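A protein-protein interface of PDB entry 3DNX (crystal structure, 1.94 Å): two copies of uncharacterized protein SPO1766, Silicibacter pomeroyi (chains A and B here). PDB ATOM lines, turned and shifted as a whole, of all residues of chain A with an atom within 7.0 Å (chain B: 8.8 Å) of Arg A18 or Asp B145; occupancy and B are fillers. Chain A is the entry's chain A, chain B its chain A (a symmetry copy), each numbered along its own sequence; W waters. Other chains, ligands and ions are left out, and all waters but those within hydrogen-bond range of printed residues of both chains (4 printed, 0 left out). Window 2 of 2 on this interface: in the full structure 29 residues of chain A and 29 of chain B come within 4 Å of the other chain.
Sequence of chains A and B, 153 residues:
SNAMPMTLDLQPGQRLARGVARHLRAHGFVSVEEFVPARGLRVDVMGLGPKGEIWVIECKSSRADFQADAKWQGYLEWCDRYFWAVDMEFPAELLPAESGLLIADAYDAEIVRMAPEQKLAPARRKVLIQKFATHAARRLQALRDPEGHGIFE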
ATOM      1  N   LEU A   8       7.504 -13.972 -17.276  1.00  0.00           N
ATOM      2  CA  LEU A   8       7.245 -14.338 -15.850  1.00  0.00           C
ATOM      3  C   LEU A   8       7.494 -15.822 -15.619  1.00  0.00           C
ATOM      4  O   LEU A   8       6.900 -16.662 -16.296  1.00  0.00           O
ATOM      5  CB  LEU A   8       5.797 -14.025 -15.449  1.00  0.00           C
ATOM      6  CG  LEU A   8       5.255 -12.595 -15.569  1.00  0.00           C
ATOM      7  CD1 LEU A   8       3.923 -12.481 -14.799  1.00  0.00           C
ATOM      8  CD2 LEU A   8       6.273 -11.554 -15.079  1.00  0.00           C
ATOM      9  N   LEU A  10       6.444 -17.282 -12.790  1.00  0.00           N
ATOM     10  CA  LEU A  10       5.577 -17.472 -11.642  1.00  0.00           C
ATOM     11  C   LEU A  10       4.786 -18.753 -11.874  1.00  0.00           C
ATOM     12  O   LEU A  10       4.371 -19.039 -13.001  1.00  0.00           O
ATOM     13  CB  LEU A  10       4.578 -16.317 -11.501  1.00  0.00           C
ATOM     14  CG  LEU A  10       5.066 -14.897 -11.210  1.00  0.00           C
ATOM     15  CD1 LEU A  10       3.868 -13.953 -11.164  1.00  0.00           C
ATOM     16  CD2 LEU A  10       5.874 -14.809  -9.918  1.00  0.00           C
ATOM     17  N   GLY A  13      -0.551 -20.528  -9.213  1.00  0.00           N
ATOM     18  CA  GLY A  13      -1.144 -19.860  -8.034  1.00  0.00           C
ATOM     19  C   GLY A  13      -0.542 -18.487  -7.780  1.00  0.00           C
ATOM     20  O   GLY A  13      -1.223 -17.530  -7.336  1.00  0.00           O
ATOM     21  N   GLN A  14       0.755 -18.362  -8.059  1.00  0.00           N
ATOM     22  CA  GLN A  14       1.412 -17.096  -7.860  1.00  0.00           C
ATOM     23  C   GLN A  14       0.899 -16.063  -8.839  1.00  0.00           C
ATOM     24  O   GLN A  14       0.911 -14.879  -8.534  1.00  0.00           O
ATOM     25  CB  GLN A  14       2.935 -17.231  -7.983  1.00  0.00           C
ATOM     26  CG  GLN A  14       3.595 -17.970  -6.818  1.00  0.00           C
ATOM     27  CD  GLN A  14       5.069 -18.161  -7.021  1.00  0.00           C
ATOM     28  OE1 GLN A  14       5.509 -18.635  -8.067  1.00  0.00           O
ATOM     29  NE2 GLN A  14       5.855 -17.811  -6.001  1.00  0.00           N
ATOM     30  N   ARG A  15       0.542 -16.512 -10.032  1.00  0.00           N
ATOM     31  CA  ARG A  15      -0.007 -15.641 -11.063  1.00  0.00           C
ATOM     32  C   ARG A  15      -1.312 -15.030 -10.601  1.00  0.00           C
ATOM     33  O   ARG A  15      -1.485 -13.820 -10.649  1.00  0.00           O
ATOM     34  CB  ARG A  15      -0.192 -16.443 -12.359  1.00  0.00           C
ATOM     35  CG  ARG A  15       1.101 -16.646 -13.173  1.00  0.00           C
ATOM     36  CD  ARG A  15       0.813 -17.388 -14.463  1.00  0.00           C
ATOM     37  NE  ARG A  15       1.901 -17.285 -15.436  1.00  0.00           N
ATOM     38  CZ  ARG A  15       1.971 -16.414 -16.454  1.00  0.00           C
ATOM     39  NH1 ARG A  15       3.020 -16.456 -17.269  1.00  0.00           N
ATOM     40  NH2 ARG A  15       1.019 -15.507 -16.683  1.00  0.00           N
ATOM     41  N   LEU A  16      -2.238 -15.880 -10.164  1.00  0.00           N
ATOM     42  CA  LEU A  16      -3.517 -15.408  -9.646  1.00  0.00           C
ATOM     43  C   LEU A  16      -3.279 -14.433  -8.493  1.00  0.00           C
ATOM     44  O   LEU A  16      -3.895 -13.380  -8.464  1.00  0.00           O
ATOM     45  CB  LEU A  16      -4.415 -16.573  -9.182  1.00  0.00           C
ATOM     46  CG  LEU A  16      -4.848 -17.607 -10.229  1.00  0.00           C
ATOM     47  CD1 LEU A  16      -5.507 -18.837  -9.561  1.00  0.00           C
ATOM     48  CD2 LEU A  16      -5.797 -16.957 -11.202  1.00  0.00           C
ATOM     49  N   ALA A  17      -2.349 -14.762  -7.585  1.00  0.00           N
ATOM     50  CA  ALA A  17      -2.125 -13.922  -6.436  1.00  0.00           C
ATOM     51  C   ALA A  17      -1.598 -12.523  -6.853  1.00  0.00           C
ATOM     52  O   ALA A  17      -1.831 -11.531  -6.160  1.00  0.00           O
ATOM     53  CB  ALA A  17      -1.162 -14.572  -5.459  1.00  0.00           C
ATOM     54  N   ARG A  18      -0.816 -12.486  -7.923  1.00  0.00           N
ATOM     55  CA  ARG A  18      -0.339 -11.184  -8.465  1.00  0.00           C
ATOM     56  C   ARG A  18      -1.454 -10.309  -8.891  1.00  0.00           C
ATOM     57  O   ARG A  18      -1.508  -9.144  -8.504  1.00  0.00           O
ATOM     58  CB  ARG A  18       0.642 -11.407  -9.620  1.00  0.00           C
ATOM     59  CG  ARG A  18       1.426 -10.159 -10.089  1.00  0.00           C
ATOM     60  CD  ARG A  18       2.281 -10.705 -11.230  1.00  0.00           C
ATOM     61  NE  ARG A  18       3.280  -9.828 -11.756  1.00  0.00           N
ATOM     62  CZ  ARG A  18       3.215  -9.223 -12.937  1.00  0.00           C
ATOM     63  NH1 ARG A  18       4.247  -8.475 -13.317  1.00  0.00           N
ATOM     64  NH2 ARG A  18       2.145  -9.335 -13.730  1.00  0.00           N
ATOM     65  N   GLY A  19      -2.402 -10.883  -9.629  1.00  0.00           N
ATOM     66  CA  GLY A  19      -3.576 -10.135 -10.087  1.00  0.00           C
ATOM     67  C   GLY A  19      -4.471  -9.733  -8.974  1.00  0.00           C
ATOM     68  O   GLY A  19      -4.933  -8.582  -8.913  1.00  0.00           O
ATOM     69  N   VAL A  20      -4.643 -10.631  -7.994  1.00  0.00           N
ATOM     70  CA  VAL A  20      -5.426 -10.289  -6.822  1.00  0.00           C
ATOM     71  C   VAL A  20      -4.829  -9.091  -6.056  1.00  0.00           C
ATOM     72  O   VAL A  20      -5.575  -8.145  -5.666  1.00  0.00           O
ATOM     73  CB  VAL A  20      -5.609 -11.536  -5.862  1.00  0.00           C
ATOM     74  CG1 VAL A  20      -6.270 -11.098  -4.569  1.00  0.00           C
ATOM     75  CG2 VAL A  20      -6.439 -12.643  -6.553  1.00  0.00           C
ATOM     76  N   ALA A  21      -3.509  -9.153  -5.817  1.00  0.00           N
ATOM     77  CA  ALA A  21      -2.784  -8.097  -5.106  1.00  0.00           C
ATOM     78  C   ALA A  21      -2.896  -6.723  -5.826  1.00  0.00           C
ATOM     79  O   ALA A  21      -3.071  -5.689  -5.157  1.00  0.00           O
ATOM     80  CB  ALA A  21      -1.350  -8.483  -4.900  1.00  0.00           C
ATOM     81  N   ARG A  22      -2.772  -6.735  -7.145  1.00  0.00           N
ATOM     82  CA  ARG A  22      -2.941  -5.484  -7.961  1.00  0.00           C
ATOM     83  C   ARG A  22      -4.292  -4.920  -7.707  1.00  0.00           C
ATOM     84  O   ARG A  22      -4.433  -3.719  -7.465  1.00  0.00           O
ATOM     85  CB  ARG A  22      -2.757  -5.749  -9.442  1.00  0.00           C
ATOM     86  CG  ARG A  22      -1.368  -6.023  -9.837  1.00  0.00           C
ATOM     87  CD  ARG A  22      -1.249  -6.439 -11.295  1.00  0.00           C
ATOM     88  NE  ARG A  22       0.138  -6.381 -11.731  1.00  0.00           N
ATOM     89  CZ  ARG A  22       0.534  -6.066 -12.963  1.00  0.00           C
ATOM     90  NH1 ARG A  22      -0.333  -5.849 -13.952  1.00  0.00           N
ATOM     91  NH2 ARG A  22       1.816  -6.018 -13.234  1.00  0.00           N
ATOM     92  N   HIS A  23      -5.333  -5.784  -7.754  1.00  0.00           N
ATOM     93  CA  HIS A  23      -6.706  -5.311  -7.652  1.00  0.00           C
ATOM     94  C   HIS A  23      -7.053  -4.815  -6.258  1.00  0.00           C
ATOM     95  O   HIS A  23      -7.700  -3.762  -6.103  1.00  0.00           O
ATOM     96  CB  HIS A  23      -7.701  -6.424  -8.099  1.00  0.00           C
ATOM     97  CG  HIS A  23      -9.120  -5.950  -8.191  1.00  0.00           C
ATOM     98  ND1 HIS A  23      -9.505  -4.935  -9.039  1.00  0.00           N
ATOM     99  CD2 HIS A  23     -10.226  -6.283  -7.475  1.00  0.00           C
ATOM    100  CE1 HIS A  23     -10.791  -4.713  -8.893  1.00  0.00           C
ATOM    101  NE2 HIS A  23     -11.251  -5.509  -7.947  1.00  0.00           N
ATOM    102  N   ARG A  25      -4.959  -3.507  -4.200  1.00  0.00           N
ATOM    103  CA  ARG A  25      -4.223  -2.245  -4.007  1.00  0.00           C
ATOM    104  C   ARG A  25      -4.947  -1.069  -4.715  1.00  0.00           C
ATOM    105  O   ARG A  25      -5.028   0.058  -4.178  1.00  0.00           O
ATOM    106  CB  ARG A  25      -2.765  -2.401  -4.430  1.00  0.00           C
ATOM    107  CG  ARG A  25      -1.905  -1.134  -4.281  1.00  0.00           C
ATOM    108  CD  ARG A  25      -0.536  -1.286  -4.886  1.00  0.00           C
ATOM    109  NE  ARG A  25       0.124  -0.014  -4.689  1.00  0.00           N
ATOM    110  CZ  ARG A  25       1.352   0.173  -4.217  1.00  0.00           C
ATOM    111  NH1 ARG A  25       2.160  -0.852  -3.939  1.00  0.00           N
ATOM    112  NH2 ARG A  25       1.773   1.425  -4.046  1.00  0.00           N
ATOM    113  N   GLU A  33       1.359 -12.513   0.704  1.00  0.00           N
ATOM    114  CA  GLU A  33       1.187 -13.862   0.257  1.00  0.00           C
ATOM    115  C   GLU A  33       1.699 -14.905   1.253  1.00  0.00           C
ATOM    116  O   GLU A  33       2.622 -14.665   2.053  1.00  0.00           O
ATOM    117  CB  GLU A  33       1.900 -14.055  -1.085  1.00  0.00           C
ATOM    118  CG  GLU A  33       1.214 -13.467  -2.270  1.00  0.00           C
ATOM    119  CD  GLU A  33       1.869 -13.923  -3.602  1.00  0.00           C
ATOM    120  OE1 GLU A  33       2.081 -15.168  -3.820  1.00  0.00           O
ATOM    121  OE2 GLU A  33       2.145 -13.047  -4.447  1.00  0.00           O
ATOM    122  N   VAL A  45      -3.458 -15.547  -0.159  1.00  0.00           N
ATOM    123  CA  VAL A  45      -3.372 -14.112  -0.024  1.00  0.00           C
ATOM    124  C   VAL A  45      -4.175 -13.687   1.201  1.00  0.00           C
ATOM    125  O   VAL A  45      -5.326 -14.104   1.381  1.00  0.00           O
ATOM    126  CB  VAL A  45      -3.874 -13.370  -1.283  1.00  0.00           C
ATOM    127  CG1 VAL A  45      -3.863 -11.834  -1.060  1.00  0.00           C
ATOM    128  CG2 VAL A  45      -3.007 -13.724  -2.485  1.00  0.00           C
ATOM    129  N   CYS A  59      -6.327 -18.915  -3.886  1.00  0.00           N
ATOM    130  CA  CYS A  59      -6.082 -18.863  -5.308  1.00  0.00           C
ATOM    131  C   CYS A  59      -5.962 -20.273  -5.836  1.00  0.00           C
ATOM    132  O   CYS A  59      -4.953 -20.920  -5.660  1.00  0.00           O
ATOM    133  CB  CYS A  59      -4.822 -18.043  -5.609  1.00  0.00           C
ATOM    134  SG  CYS A  59      -4.939 -16.339  -5.019  1.00  0.00           S
ATOM    135  N   ALA A 104      -9.411 -13.861 -11.778  1.00  0.00           N
ATOM    136  CA  ALA A 104      -8.091 -13.255 -11.767  1.00  0.00           C
ATOM    137  C   ALA A 104      -7.199 -13.869 -12.848  1.00  0.00           C
ATOM    138  O   ALA A 104      -7.504 -14.946 -13.407  1.00  0.00           O
ATOM    139  CB  ALA A 104      -7.436 -13.433 -10.371  1.00  0.00           C
ATOM    140  N   ASP A 105      -6.133 -13.134 -13.161  1.00  0.00           N
ATOM    141  CA  ASP A 105      -4.973 -13.656 -13.905  1.00  0.00           C
ATOM    142  C   ASP A 105      -3.734 -12.942 -13.383  1.00  0.00           C
ATOM    143  O   ASP A 105      -3.824 -12.309 -12.356  1.00  0.00           O
ATOM    144  CB  ASP A 105      -5.135 -13.537 -15.438  1.00  0.00           C
ATOM    145  CG  ASP A 105      -5.255 -12.089 -15.951  1.00  0.00           C
ATOM    146  OD1 ASP A 105      -4.950 -11.095 -15.259  1.00  0.00           O
ATOM    147  OD2 ASP A 105      -5.658 -11.936 -17.116  1.00  0.00           O
ATOM    148  N   ALA A 106      -2.594 -13.024 -14.077  1.00  0.00           N
ATOM    149  CA  ALA A 106      -1.369 -12.429 -13.549  1.00  0.00           C
ATOM    150  C   ALA A 106      -1.428 -10.921 -13.548  1.00  0.00           C
ATOM    151  O   ALA A 106      -0.606 -10.323 -12.896  1.00  0.00           O
ATOM    152  CB  ALA A 106      -0.112 -12.903 -14.324  1.00  0.00           C
ATOM    153  N   TYR A 107      -2.400 -10.308 -14.236  1.00  0.00           N
ATOM    154  CA  TYR A 107      -2.339  -8.893 -14.483  1.00  0.00           C
ATOM    155  C   TYR A 107      -3.400  -8.060 -13.796  1.00  0.00           C
ATOM    156  O   TYR A 107      -3.253  -6.835 -13.696  1.00  0.00           O
ATOM    157  CB  TYR A 107      -2.437  -8.646 -15.976  1.00  0.00           C
ATOM    158  CG  TYR A 107      -1.411  -9.464 -16.723  1.00  0.00           C
ATOM    159  CD1 TYR A 107      -0.084  -9.112 -16.671  1.00  0.00           C
ATOM    160  CD2 TYR A 107      -1.769 -10.634 -17.401  1.00  0.00           C
ATOM    161  CE1 TYR A 107       0.887  -9.836 -17.355  1.00  0.00           C
ATOM    162  CE2 TYR A 107      -0.807 -11.388 -18.068  1.00  0.00           C
ATOM    163  CZ  TYR A 107       0.519 -10.974 -18.042  1.00  0.00           C
ATOM    164  OH  TYR A 107       1.512 -11.679 -18.677  1.00  0.00           O
ATOM    165  N   ASP A 108      -4.459  -8.708 -13.345  1.00  0.00           N
ATOM    166  CA  ASP A 108      -5.602  -8.007 -12.731  1.00  0.00           C
ATOM    167  C   ASP A 108      -6.574  -9.014 -12.147  1.00  0.00           C
ATOM    168  O   ASP A 108      -6.358 -10.217 -12.241  1.00  0.00           O
ATOM    169  CB  ASP A 108      -6.294  -7.139 -13.754  1.00  0.00           C
ATOM    170  CG  ASP A 108      -7.054  -5.933 -13.138  1.00  0.00           C
ATOM    171  OD1 ASP A 108      -7.201  -5.780 -11.899  1.00  0.00           O
ATOM    172  OD2 ASP A 108      -7.507  -5.138 -13.951  1.00  0.00           O
ATOM    173  N   ALA A 109      -7.634  -8.516 -11.511  1.00  0.00           N
ATOM    174  CA  ALA A 109      -8.684  -9.332 -10.966  1.00  0.00           C
ATOM    175  C   ALA A 109      -9.968  -8.535 -10.820  1.00  0.00           C
ATOM    176  O   ALA A 109      -9.967  -7.301 -10.873  1.00  0.00           O
ATOM    177  CB  ALA A 109      -8.278  -9.931  -9.630  1.00  0.00           C
ATOM    178  N   ARG B 138       2.552  -2.080   1.004  1.00  0.00           N
ATOM    179  CA  ARG B 138       2.595  -1.318  -0.247  1.00  0.00           C
ATOM    180  C   ARG B 138       3.971  -1.377  -0.867  1.00  0.00           C
ATOM    181  O   ARG B 138       4.112  -1.675  -2.046  1.00  0.00           O
ATOM    182  CB  ARG B 138       2.215   0.164  -0.057  1.00  0.00           C
ATOM    183  CG  ARG B 138       0.765   0.414  -0.162  1.00  0.00           C
ATOM    184  CD  ARG B 138       0.427   1.944  -0.096  1.00  0.00           C
ATOM    185  NE  ARG B 138      -1.035   2.077  -0.096  1.00  0.00           N
ATOM    186  CZ  ARG B 138      -1.758   2.816   0.762  1.00  0.00           C
ATOM    187  NH1 ARG B 138      -1.174   3.574   1.703  1.00  0.00           N
ATOM    188  NH2 ARG B 138      -3.088   2.819   0.656  1.00  0.00           N
ATOM    189  N   ARG B 139       5.000  -1.028  -0.071  1.00  0.00           N
ATOM    190  CA  ARG B 139       6.367  -1.015  -0.579  1.00  0.00           C
ATOM    191  C   ARG B 139       6.798  -2.372  -1.066  1.00  0.00           C
ATOM    192  O   ARG B 139       7.516  -2.478  -2.041  1.00  0.00           O
ATOM    193  CB  ARG B 139       7.358  -0.550   0.514  1.00  0.00           C
ATOM    194  CG  ARG B 139       7.036   0.772   1.120  1.00  0.00           C
ATOM    195  CD  ARG B 139       7.280   1.896   0.233  1.00  0.00           C
ATOM    196  NE  ARG B 139       7.226   3.155   0.993  1.00  0.00           N
ATOM    197  CZ  ARG B 139       6.109   3.839   1.295  1.00  0.00           C
ATOM    198  NH1 ARG B 139       4.897   3.403   0.934  1.00  0.00           N
ATOM    199  NH2 ARG B 139       6.208   4.978   1.970  1.00  0.00           N
ATOM    200  N   LEU B 140       6.436  -3.410  -0.330  1.00  0.00           N
ATOM    201  CA  LEU B 140       6.735  -4.782  -0.727  1.00  0.00           C
ATOM    202  C   LEU B 140       6.121  -5.127  -2.077  1.00  0.00           C
ATOM    203  O   LEU B 140       6.809  -5.613  -2.995  1.00  0.00           O
ATOM    204  CB  LEU B 140       6.228  -5.734   0.331  1.00  0.00           C
ATOM    205  CG  LEU B 140       6.324  -7.243   0.098  1.00  0.00           C
ATOM    206  CD1 LEU B 140       7.720  -7.658  -0.286  1.00  0.00           C
ATOM    207  CD2 LEU B 140       5.841  -7.932   1.361  1.00  0.00           C
ATOM    208  N   GLN B 141       4.826  -4.841  -2.226  1.00  0.00           N
ATOM    209  CA  GLN B 141       4.147  -5.137  -3.486  1.00  0.00           C
ATOM    210  C   GLN B 141       4.790  -4.390  -4.675  1.00  0.00           C
ATOM    211  O   GLN B 141       4.926  -4.947  -5.745  1.00  0.00           O
ATOM    212  CB  GLN B 141       2.630  -4.899  -3.386  1.00  0.00           C
ATOM    213  CG  GLN B 141       1.811  -5.461  -4.587  1.00  0.00           C
ATOM    214  CD  GLN B 141       1.628  -4.421  -5.680  1.00  0.00           C
ATOM    215  OE1 GLN B 141       2.082  -3.267  -5.522  1.00  0.00           O
ATOM    216  NE2 GLN B 141       0.992  -4.808  -6.797  1.00  0.00           N
ATOM    217  N   ALA B 142       5.180  -3.144  -4.464  1.00  0.00           N
ATOM    218  CA  ALA B 142       5.798  -2.353  -5.490  1.00  0.00           C
ATOM    219  C   ALA B 142       7.192  -2.890  -5.920  1.00  0.00           C
ATOM    220  O   ALA B 142       7.582  -2.735  -7.084  1.00  0.00           O
ATOM    221  CB  ALA B 142       5.873  -0.918  -5.040  1.00  0.00           C
ATOM    222  N   LEU B 143       7.947  -3.482  -5.000  1.00  0.00           N
ATOM    223  CA  LEU B 143       9.242  -4.086  -5.333  1.00  0.00           C
ATOM    224  C   LEU B 143       9.050  -5.376  -6.070  1.00  0.00           C
ATOM    225  O   LEU B 143       9.719  -5.628  -7.065  1.00  0.00           O
ATOM    226  CB  LEU B 143      10.081  -4.329  -4.069  1.00  0.00           C
ATOM    227  CG  LEU B 143      10.836  -3.149  -3.505  1.00  0.00           C
ATOM    228  CD1 LEU B 143      11.714  -3.616  -2.290  1.00  0.00           C
ATOM    229  CD2 LEU B 143      11.684  -2.445  -4.590  1.00  0.00           C
ATOM    230  N   ARG B 144       8.061  -6.165  -5.651  1.00  0.00           N
ATOM    231  CA  ARG B 144       7.757  -7.435  -6.333  1.00  0.00           C
ATOM    232  C   ARG B 144       7.071  -7.326  -7.670  1.00  0.00           C
ATOM    233  O   ARG B 144       7.191  -8.221  -8.504  1.00  0.00           O
ATOM    234  CB  ARG B 144       6.943  -8.330  -5.412  1.00  0.00           C
ATOM    235  CG  ARG B 144       7.611  -8.499  -4.094  1.00  0.00           C
ATOM    236  CD  ARG B 144       7.527  -9.876  -3.508  1.00  0.00           C
ATOM    237  NE  ARG B 144       6.180 -10.375  -3.443  1.00  0.00           N
ATOM    238  CZ  ARG B 144       5.712 -11.437  -4.115  1.00  0.00           C
ATOM    239  NH1 ARG B 144       4.447 -11.770  -3.969  1.00  0.00           N
ATOM    240  NH2 ARG B 144       6.478 -12.181  -4.926  1.00  0.00           N
ATOM    241  N   ASP B 145       6.365  -6.210  -7.893  1.00  0.00           N
ATOM    242  CA  ASP B 145       5.558  -6.021  -9.084  1.00  0.00           C
ATOM    243  C   ASP B 145       5.589  -4.524  -9.402  1.00  0.00           C
ATOM    244  O   ASP B 145       4.620  -3.843  -9.172  1.00  0.00           O
ATOM    245  CB  ASP B 145       4.133  -6.514  -8.788  1.00  0.00           C
ATOM    246  CG  ASP B 145       3.190  -6.440  -9.974  1.00  0.00           C
ATOM    247  OD1 ASP B 145       3.603  -6.114 -11.125  1.00  0.00           O
ATOM    248  OD2 ASP B 145       1.983  -6.691  -9.743  1.00  0.00           O
ATOM    249  N   PRO B 146       6.721  -4.029  -9.940  1.00  0.00           N
ATOM    250  CA  PRO B 146       6.949  -2.603 -10.179  1.00  0.00           C
ATOM    251  C   PRO B 146       5.843  -1.892 -10.965  1.00  0.00           C
ATOM    252  O   PRO B 146       5.528  -0.728 -10.657  1.00  0.00           O
ATOM    253  CB  PRO B 146       8.266  -2.570 -10.947  1.00  0.00           C
ATOM    254  CG  PRO B 146       8.928  -3.878 -10.690  1.00  0.00           C
ATOM    255  CD  PRO B 146       7.911  -4.852 -10.261  1.00  0.00           C
ATOM    256  N   GLU B 147       5.261  -2.580 -11.956  1.00  0.00           N
ATOM    257  CA  GLU B 147       4.245  -1.963 -12.841  1.00  0.00           C
ATOM    258  C   GLU B 147       2.839  -2.068 -12.238  1.00  0.00           C
ATOM    259  O   GLU B 147       1.912  -1.405 -12.693  1.00  0.00           O
ATOM    260  CB  GLU B 147       4.247  -2.646 -14.229  1.00  0.00           C
ATOM    261  CG  GLU B 147       5.293  -2.198 -15.309  1.00  0.00           C
ATOM    262  CD  GLU B 147       6.312  -1.114 -14.906  1.00  0.00           C
ATOM    263  OE1 GLU B 147       5.888   0.042 -14.647  1.00  0.00           O
ATOM    264  OE2 GLU B 147       7.552  -1.398 -14.918  1.00  0.00           O
ATOM    265  N   GLY B 148       2.687  -2.869 -11.200  1.00  0.00           N
ATOM    266  CA  GLY B 148       1.391  -3.263 -10.699  1.00  0.00           C
ATOM    267  C   GLY B 148       0.626  -2.325  -9.771  1.00  0.00           C
ATOM    268  O   GLY B 148      -0.039  -2.795  -8.796  1.00  0.00           O
ATOM    269  N   HIS B 149       0.707  -1.019 -10.077  1.00  0.00           N
ATOM    270  CA  HIS B 149      -0.162  -0.020  -9.438  1.00  0.00           C
ATOM    271  C   HIS B 149      -0.319   1.220 -10.333  1.00  0.00           C
ATOM    272  O   HIS B 149       0.382   1.373 -11.303  1.00  0.00           O
ATOM    273  CB  HIS B 149       0.364   0.362  -8.050  1.00  0.00           C
ATOM    274  CG  HIS B 149       1.672   1.086  -8.063  1.00  0.00           C
ATOM    275  ND1 HIS B 149       2.892   0.428  -8.031  1.00  0.00           N
ATOM    276  CD2 HIS B 149       1.954   2.410  -8.094  1.00  0.00           C
ATOM    277  CE1 HIS B 149       3.867   1.325  -8.019  1.00  0.00           C
ATOM    278  NE2 HIS B 149       3.321   2.536  -8.062  1.00  0.00           N
ATOM    279  N   GLY B 150      -1.284   2.061 -10.027  1.00  0.00           N
ATOM    280  CA  GLY B 150      -1.493   3.269 -10.779  1.00  0.00           C
ATOM    281  C   GLY B 150      -0.995   4.508 -10.058  1.00  0.00           C
ATOM    282  O   GLY B 150      -0.637   4.486  -8.863  1.00  0.00           O
HETATM  283  O   HOH W   1      -2.732  -1.782  -8.028  1.00  0.00           O
HETATM  284  O   HOH W   2       5.579  -5.317 -12.955  1.00  0.00           O
HETATM  285  O   HOH W   3       5.599  -9.913  -9.922  1.00  0.00           O
HETATM  286  O   HOH W   4       0.825  -7.648  -7.578  1.00  0.00           O
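No residue of chain B comes within 4 Å of Ala A17. Gly A19 touches none of the printed residues of chain B. Of the printed residues of chain B, Arg A22 touches Asp B145 and Gly B148. Of the printed residues of chain B, Glu A33 touches Arg B144 (2.7 Å). Of the printed residues of chain A, Arg B138 touches Arg A25 (2.8 Å). Arg B139 touches none of the printed residues of chain A. Of the printed residues of chain A, Ala B142 touches Arg A25. Asp B145 touches two residues of chain A. The nearest residue of chain A that does not touch Asp B145 is Ala A106 (5.5 Å). The nearest printed residue of chain B that does not touch Arg A25 is Gly B148 (4.2 Å).
Printed residues of chain B that touch a printed residue of chain A: Arg B138, Gln B141, Ala B142, Arg B144, Asp B145, Gly B148 and His B149. Hydrophobic or aromatic side chains of chain B within 4 Å of the printed part of chain A: Ala B142 and His B149. Among the printed residues, 8 pairs touch across the chains.
NH2 of Arg A18 lies within hydrogen-bond range of O of Ala A106 (3.0 Å). The guanidinium group (NH1) of Arg A22 is in hydrogen-bond range of the backbone carbonyl oxygen (O) of Tyr A107. NE2 of Gln B141 sits at hydrogen-bond distance from O of Gly B148. OD1 of Asp B145 lies within hydrogen-bond range of N of Gly B148, 3.4 Å away.
Water W4 lies within hydrogen-bond range of OD2 of Asp B145 (2.6 Å), O of Arg A18 (2.9 Å) and NE2 of Gln B141 (3.0 Å). Water W1 bridges the backbone carbonyl oxygen (O) of Arg A22 (2.6 Å) and the backbone carbonyl oxygen (O) of Gly B148 (3.0 Å). Water W3 lies within hydrogen-bond range of the backbone carbonyl oxygen (O) of Arg B144 (2.7 Å) and the guanidinium group (NE) of Arg A18 (3.0 Å). Water W2 lies within hydrogen-bond range of the side-chain carboxylate (OD1) of Asp B145 (2.8 Å), the backbone NH (N) of Glu B147 (2.9 Å) and the guanidinium group (NH1) of Arg A18 (3.4 Å).
Among the printed residues, pairs that only touch across the chains: Arg A25 with His B149, Arg A22 with Gly B148 and Arg A25 with Ala B142.
No position is printed for both chains. Of the 8 pairs that touch across the chains among the printed residues, none has its exchanged pair printed and touching as well.
The guanidinium group of Arg A18 lies within salt-bridge range of the side-chain carboxylate of Asp B145, at 3.3 Å. The guanidinium group (NE) of Arg A22 is in salt-bridge range of the side-chain carboxylate (OD2) of Asp B145 (2.7 Å). The guanidinium group of Arg A25 is in hydrogen-bond range of the backbone carbonyl oxygen of Arg B138, at 2.8 Å. The guanidinium group (NH1) of Arg A25 is in hydrogen-bond range of the side-chain amide oxygen (OE1) of Gln B141, at 2.9 Å. OE2 of Glu A33 lies within salt-bridge range of NH1 of Arg B144, at 2.7 Å.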
